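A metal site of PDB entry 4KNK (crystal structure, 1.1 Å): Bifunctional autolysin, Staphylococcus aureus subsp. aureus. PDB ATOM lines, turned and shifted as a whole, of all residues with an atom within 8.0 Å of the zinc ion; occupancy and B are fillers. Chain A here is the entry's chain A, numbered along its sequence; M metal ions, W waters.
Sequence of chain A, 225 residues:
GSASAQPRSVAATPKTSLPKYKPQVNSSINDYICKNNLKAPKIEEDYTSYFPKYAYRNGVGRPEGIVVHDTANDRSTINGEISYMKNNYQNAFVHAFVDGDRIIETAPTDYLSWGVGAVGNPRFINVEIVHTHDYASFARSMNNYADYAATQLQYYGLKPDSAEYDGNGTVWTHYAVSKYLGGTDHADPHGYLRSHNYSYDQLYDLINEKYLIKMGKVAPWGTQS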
ATOM      1  N   VAL A  67     -18.290  -0.104 -17.934  1.00  0.00           N
ATOM      2  CA  VAL A  67     -18.737   0.208 -16.583  1.00  0.00           C
ATOM      3  C   VAL A  67     -20.253   0.196 -16.485  1.00  0.00           C
ATOM      4  O   VAL A  67     -20.963   0.722 -17.349  1.00  0.00           O
ATOM      5  CB  VAL A  67     -18.236   1.613 -16.136  1.00  0.00           C
ATOM      6  CG1 VAL A  67     -18.682   1.925 -14.686  1.00  0.00           C
ATOM      7  CG2 VAL A  67     -16.717   1.692 -16.210  1.00  0.00           C
ATOM      8  N   VAL A  68     -20.742  -0.418 -15.402  1.00  0.00           N
ATOM      9  CA  VAL A  68     -22.154  -0.400 -15.039  1.00  0.00           C
ATOM     10  C   VAL A  68     -22.421   0.782 -14.118  1.00  0.00           C
ATOM     11  O   VAL A  68     -21.892   0.849 -13.006  1.00  0.00           O
ATOM     12  CB  VAL A  68     -22.560  -1.703 -14.307  1.00  0.00           C
ATOM     13  CG1 VAL A  68     -24.067  -1.759 -14.221  1.00  0.00           C
ATOM     14  CG2 VAL A  68     -22.015  -2.975 -15.000  1.00  0.00           C
ATOM     15  N   HIS A  69     -23.294   1.676 -14.584  1.00  0.00           N
ATOM     16  CA  HIS A  69     -23.787   2.824 -13.831  1.00  0.00           C
ATOM     17  C   HIS A  69     -25.297   2.735 -13.698  1.00  0.00           C
ATOM     18  O   HIS A  69     -25.965   2.091 -14.514  1.00  0.00           O
ATOM     19  CB  HIS A  69     -23.529   4.130 -14.581  1.00  0.00           C
ATOM     20  CG  HIS A  69     -22.109   4.465 -14.843  1.00  0.00           C
ATOM     21  ND1 HIS A  69     -21.356   5.203 -13.957  1.00  0.00           N
ATOM     22  CD2 HIS A  69     -21.318   4.211 -15.911  1.00  0.00           C
ATOM     23  CE1 HIS A  69     -20.159   5.388 -14.487  1.00  0.00           C
ATOM     24  NE2 HIS A  69     -20.107   4.785 -15.673  1.00  0.00           N
ATOM     25  N   ASP A  70     -25.855   3.453 -12.715  1.00  0.00           N
ATOM     26  CA  ASP A  70     -27.263   3.773 -12.779  1.00  0.00           C
ATOM     27  C   ASP A  70     -27.436   5.264 -12.538  1.00  0.00           C
ATOM     28  O   ASP A  70     -26.570   5.903 -11.933  1.00  0.00           O
ATOM     29  CB  ASP A  70     -28.151   2.918 -11.861  1.00  0.00           C
ATOM     30  CG  ASP A  70     -28.038   3.324 -10.403  1.00  0.00           C
ATOM     31  OD1 ASP A  70     -28.809   4.222  -9.974  1.00  0.00           O
ATOM     32  OD2 ASP A  70     -27.202   2.729  -9.691  1.00  0.00           O
ATOM     33  N   THR A  71     -28.551   5.819 -12.987  1.00  0.00           N
ATOM     34  CA  THR A  71     -28.722   7.268 -13.002  1.00  0.00           C
ATOM     35  C   THR A  71     -28.930   7.887 -11.620  1.00  0.00           C
ATOM     36  O   THR A  71     -28.862   9.109 -11.477  1.00  0.00           O
ATOM     37  CB  THR A  71     -29.940   7.671 -13.825  1.00  0.00           C
ATOM     38  OG1 THR A  71     -31.072   7.017 -13.241  1.00  0.00           O
ATOM     39  CG2 THR A  71     -29.778   7.280 -15.281  1.00  0.00           C
ATOM     40  N   ALA A  72     -29.204   7.073 -10.602  1.00  0.00           N
ATOM     41  CA  ALA A  72     -29.503   7.574  -9.256  1.00  0.00           C
ATOM     42  C   ALA A  72     -30.672   8.548  -9.283  1.00  0.00           C
ATOM     43  O   ALA A  72     -30.764   9.479  -8.461  1.00  0.00           O
ATOM     44  CB  ALA A  72     -28.262   8.228  -8.602  1.00  0.00           C
ATOM     45  N   VAL A  94     -22.077  10.022 -21.152  1.00  0.00           N
ATOM     46  CA  VAL A  94     -21.838   8.600 -21.224  1.00  0.00           C
ATOM     47  C   VAL A  94     -22.037   8.099 -22.653  1.00  0.00           C
ATOM     48  O   VAL A  94     -22.542   8.815 -23.531  1.00  0.00           O
ATOM     49  CB  VAL A  94     -22.723   7.794 -20.252  1.00  0.00           C
ATOM     50  CG1 VAL A  94     -22.381   8.180 -18.810  1.00  0.00           C
ATOM     51  CG2 VAL A  94     -24.214   7.987 -20.558  1.00  0.00           C
ATOM     52  N   GLY A 115     -17.752   9.869 -17.837  1.00  0.00           N
ATOM     53  CA  GLY A 115     -18.730   9.246 -16.975  1.00  0.00           C
ATOM     54  C   GLY A 115     -18.242   8.678 -15.659  1.00  0.00           C
ATOM     55  O   GLY A 115     -19.084   8.318 -14.827  1.00  0.00           O
ATOM     56  N   VAL A 116     -16.926   8.549 -15.456  1.00  0.00           N
ATOM     57  CA  VAL A 116     -16.445   7.787 -14.303  1.00  0.00           C
ATOM     58  C   VAL A 116     -15.133   8.342 -13.722  1.00  0.00           C
ATOM     59  O   VAL A 116     -14.424   7.644 -12.989  1.00  0.00           O
ATOM     60  CB  VAL A 116     -16.418   6.253 -14.629  1.00  0.00           C
ATOM     61  CG1 VAL A 116     -15.177   5.870 -15.446  1.00  0.00           C
ATOM     62  CG2 VAL A 116     -16.567   5.389 -13.385  1.00  0.00           C
ATOM     63  N   ASN A 126     -18.811   3.739 -20.811  1.00  0.00           N
ATOM     64  CA  ASN A 126     -19.719   4.052 -19.697  1.00  0.00           C
ATOM     65  C   ASN A 126     -21.162   3.889 -20.155  1.00  0.00           C
ATOM     66  O   ASN A 126     -21.594   4.585 -21.088  1.00  0.00           O
ATOM     67  CB  ASN A 126     -19.498   5.498 -19.234  1.00  0.00           C
ATOM     68  CG  ASN A 126     -18.177   5.674 -18.511  1.00  0.00           C
ATOM     69  OD1 ASN A 126     -17.949   5.063 -17.459  1.00  0.00           O
ATOM     70  ND2 ASN A 126     -17.308   6.519 -19.060  1.00  0.00           N
ATOM     71  N   VAL A 127     -21.924   3.048 -19.461  1.00  0.00           N
ATOM     72  CA  VAL A 127     -23.332   2.814 -19.809  1.00  0.00           C
ATOM     73  C   VAL A 127     -24.202   3.001 -18.569  1.00  0.00           C
ATOM     74  O   VAL A 127     -23.872   2.448 -17.496  1.00  0.00           O
ATOM     75  CB  VAL A 127     -23.535   1.407 -20.377  1.00  0.00           C
ATOM     76  CG1 VAL A 127     -25.000   1.177 -20.772  1.00  0.00           C
ATOM     77  CG2 VAL A 127     -22.635   1.200 -21.596  1.00  0.00           C
ATOM     78  N   GLU A 128     -25.283   3.765 -18.727  1.00  0.00           N
ATOM     79  CA  GLU A 128     -26.206   4.077 -17.646  1.00  0.00           C
ATOM     80  C   GLU A 128     -27.499   3.290 -17.723  1.00  0.00           C
ATOM     81  O   GLU A 128     -28.145   3.260 -18.767  1.00  0.00           O
ATOM     82  CB  GLU A 128     -26.626   5.540 -17.742  1.00  0.00           C
ATOM     83  CG  GLU A 128     -25.632   6.529 -17.351  1.00  0.00           C
ATOM     84  CD  GLU A 128     -25.534   6.692 -15.858  1.00  0.00           C
ATOM     85  OE1 GLU A 128     -26.296   6.027 -15.123  1.00  0.00           O
ATOM     86  OE2 GLU A 128     -24.666   7.478 -15.443  1.00  0.00           O
ATOM     87  N   THR A 173     -18.049  -2.004 -12.096  1.00  0.00           N
ATOM     88  CA  THR A 173     -19.069  -1.098 -11.590  1.00  0.00           C
ATOM     89  C   THR A 173     -18.423   0.260 -11.337  1.00  0.00           C
ATOM     90  O   THR A 173     -17.204   0.361 -11.177  1.00  0.00           O
ATOM     91  CB  THR A 173     -19.678  -1.616 -10.280  1.00  0.00           C
ATOM     92  OG1 THR A 173     -18.631  -1.815  -9.325  1.00  0.00           O
ATOM     93  CG2 THR A 173     -20.413  -2.925 -10.514  1.00  0.00           C
ATOM     94  N   HIS A 174     -19.249   1.296 -11.239  1.00  0.00           N
ATOM     95  CA  HIS A 174     -18.724   2.583 -10.814  1.00  0.00           C
ATOM     96  C   HIS A 174     -18.061   2.398  -9.427  1.00  0.00           C
ATOM     97  O   HIS A 174     -16.975   2.937  -9.176  1.00  0.00           O
ATOM     98  CB  HIS A 174     -19.835   3.632 -10.808  1.00  0.00           C
ATOM     99  CG  HIS A 174     -19.335   5.039 -10.759  1.00  0.00           C
ATOM    100  ND1 HIS A 174     -20.021   6.082 -11.342  1.00  0.00           N
ATOM    101  CD2 HIS A 174     -18.184   5.567 -10.259  1.00  0.00           C
ATOM    102  CE1 HIS A 174     -19.336   7.202 -11.187  1.00  0.00           C
ATOM    103  NE2 HIS A 174     -18.220   6.926 -10.525  1.00  0.00           N
ATOM    104  N   TYR A 175     -18.709   1.645  -8.549  1.00  0.00           N
ATOM    105  CA  TYR A 175     -18.166   1.361  -7.219  1.00  0.00           C
ATOM    106  C   TYR A 175     -16.746   0.801  -7.320  1.00  0.00           C
ATOM    107  O   TYR A 175     -15.844   1.249  -6.614  1.00  0.00           O
ATOM    108  CB  TYR A 175     -19.064   0.350  -6.517  1.00  0.00           C
ATOM    109  CG  TYR A 175     -18.619  -0.038  -5.142  1.00  0.00           C
ATOM    110  CD1 TYR A 175     -17.721  -1.075  -4.952  1.00  0.00           C
ATOM    111  CD2 TYR A 175     -19.107   0.614  -4.028  1.00  0.00           C
ATOM    112  CE1 TYR A 175     -17.293  -1.434  -3.679  1.00  0.00           C
ATOM    113  CE2 TYR A 175     -18.701   0.273  -2.764  1.00  0.00           C
ATOM    114  CZ  TYR A 175     -17.790  -0.758  -2.598  1.00  0.00           C
ATOM    115  OH  TYR A 175     -17.391  -1.102  -1.322  1.00  0.00           O
ATOM    116  N   SER A 178     -14.248   3.462  -8.246  1.00  0.00           N
ATOM    117  CA  SER A 178     -13.981   4.259  -7.052  1.00  0.00           C
ATOM    118  C   SER A 178     -13.021   3.535  -6.100  1.00  0.00           C
ATOM    119  O   SER A 178     -12.090   4.156  -5.562  1.00  0.00           O
ATOM    120  CB  SER A 178     -15.287   4.565  -6.323  1.00  0.00           C
ATOM    121  OG  SER A 178     -16.150   5.325  -7.145  1.00  0.00           O
ATOM    122  N   THR A 184     -12.913   9.139  -8.559  1.00  0.00           N
ATOM    123  CA  THR A 184     -14.367   9.230  -8.452  1.00  0.00           C
ATOM    124  C   THR A 184     -14.765   8.550  -7.158  1.00  0.00           C
ATOM    125  O   THR A 184     -13.971   7.764  -6.613  1.00  0.00           O
ATOM    126  CB  THR A 184     -15.049   8.566  -9.678  1.00  0.00           C
ATOM    127  OG1 THR A 184     -16.450   8.800  -9.624  1.00  0.00           O
ATOM    128  CG2 THR A 184     -14.781   7.058  -9.720  1.00  0.00           C
ATOM    129  N   HIS A 186     -18.373   7.466  -6.502  1.00  0.00           N
ATOM    130  CA  HIS A 186     -19.746   6.963  -6.559  1.00  0.00           C
ATOM    131  C   HIS A 186     -19.819   5.465  -6.320  1.00  0.00           C
ATOM    132  O   HIS A 186     -18.841   4.743  -6.526  1.00  0.00           O
ATOM    133  CB  HIS A 186     -20.400   7.308  -7.888  1.00  0.00           C
ATOM    134  CG  HIS A 186     -20.551   8.780  -8.111  1.00  0.00           C
ATOM    135  ND1 HIS A 186     -21.724   9.448  -7.854  1.00  0.00           N
ATOM    136  CD2 HIS A 186     -19.660   9.703  -8.530  1.00  0.00           C
ATOM    137  CE1 HIS A 186     -21.562  10.726  -8.142  1.00  0.00           C
ATOM    138  NE2 HIS A 186     -20.316  10.916  -8.552  1.00  0.00           N
ATOM    139  N   ALA A 187     -20.995   5.000  -5.924  1.00  0.00           N
ATOM    140  CA  ALA A 187     -21.161   3.614  -5.464  1.00  0.00           C
ATOM    141  C   ALA A 187     -22.149   2.797  -6.310  1.00  0.00           C
ATOM    142  O   ALA A 187     -22.455   1.646  -5.975  1.00  0.00           O
ATOM    143  CB  ALA A 187     -21.604   3.611  -4.000  1.00  0.00           C
ATOM    144  N   ASP A 188     -22.630   3.380  -7.412  1.00  0.00           N
ATOM    145  CA  ASP A 188     -23.554   2.658  -8.267  1.00  0.00           C
ATOM    146  C   ASP A 188     -22.871   1.434  -8.879  1.00  0.00           C
ATOM    147  O   ASP A 188     -21.643   1.414  -9.081  1.00  0.00           O
ATOM    148  CB  ASP A 188     -24.193   3.621  -9.297  1.00  0.00           C
ATOM    149  CG  ASP A 188     -23.203   4.546 -10.000  1.00  0.00           C
ATOM    150  OD1 ASP A 188     -22.412   5.243  -9.326  1.00  0.00           O
ATOM    151  OD2 ASP A 188     -23.261   4.619 -11.260  1.00  0.00           O
ATOM    152  N   PRO A 189     -23.648   0.389  -9.226  1.00  0.00           N
ATOM    153  CA  PRO A 189     -25.109   0.298  -9.222  1.00  0.00           C
ATOM    154  C   PRO A 189     -25.643  -0.552  -8.086  1.00  0.00           C
ATOM    155  O   PRO A 189     -26.810  -0.958  -8.136  1.00  0.00           O
ATOM    156  CB  PRO A 189     -25.374  -0.435 -10.534  1.00  0.00           C
ATOM    157  CG  PRO A 189     -24.279  -1.464 -10.528  1.00  0.00           C
ATOM    158  CD  PRO A 189     -23.060  -0.721  -9.982  1.00  0.00           C
HETATM  159 ZN    ZN M   1     -21.954   6.009 -12.057  1.00  0.00          ZN
HETATM  160  O   HOH W   1     -23.656   7.166 -12.893  1.00  0.00           O
HETATM  161  O   HOH W   2     -22.676   7.759 -10.511  1.00  0.00           O
HETATM  162  O   HOH W   3     -21.442   8.315 -13.306  1.00  0.00           O
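The backbone carbonyl oxygen (O) of Val 68 sits at hydrogen-bond distance from the backbone NH (N) of His 174. OG1 of Thr 184 lies within hydrogen-bond range of NE2 of His 174, 2.7 Å away. OG of Ser 178 sits at hydrogen-bond distance from O of His 174. The side-chain carboxylate (OD2) of Asp 188 lies close to the backbone NH (N) of Asp 70 (3.2 Å). The backbone carbonyl oxygen of Asp 188 sits at hydrogen-bond distance from the backbone NH of Tyr 175, 3.0 Å away. The backbone NH (N) of His 69 sits at hydrogen-bond distance from the backbone carbonyl oxygen (O) of Val 127, 3.1 Å away. A ring nitrogen (NE2) of His 69 lies within hydrogen-bond range of the side-chain amide oxygen (OD1) of Asn 126 (2.8 Å).
Of the 21 residues printed, 3 come within 4 Å of the zinc ion. The nearest printed residue that does not touch the zinc ion is Glu 128 (4.6 Å).
The zinc ion is bound by ND1 of His 174 (2.1 Å), OD2 of Asp 188 (2.1 Å), ND1 of His 69 (2.1 Å), water W1 (2.2 Å) and water W2 (2.4 Å). Slightly farther from the zinc ion lies water W3 (2.7 Å).
Water W1 bridges OE2 of Glu 128 (2.8 Å) and O of Asp 70 (3.3 Å). Water W2 bridges the side-chain carboxylate of Asp 188 and a ring nitrogen (ND1) of His 186.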
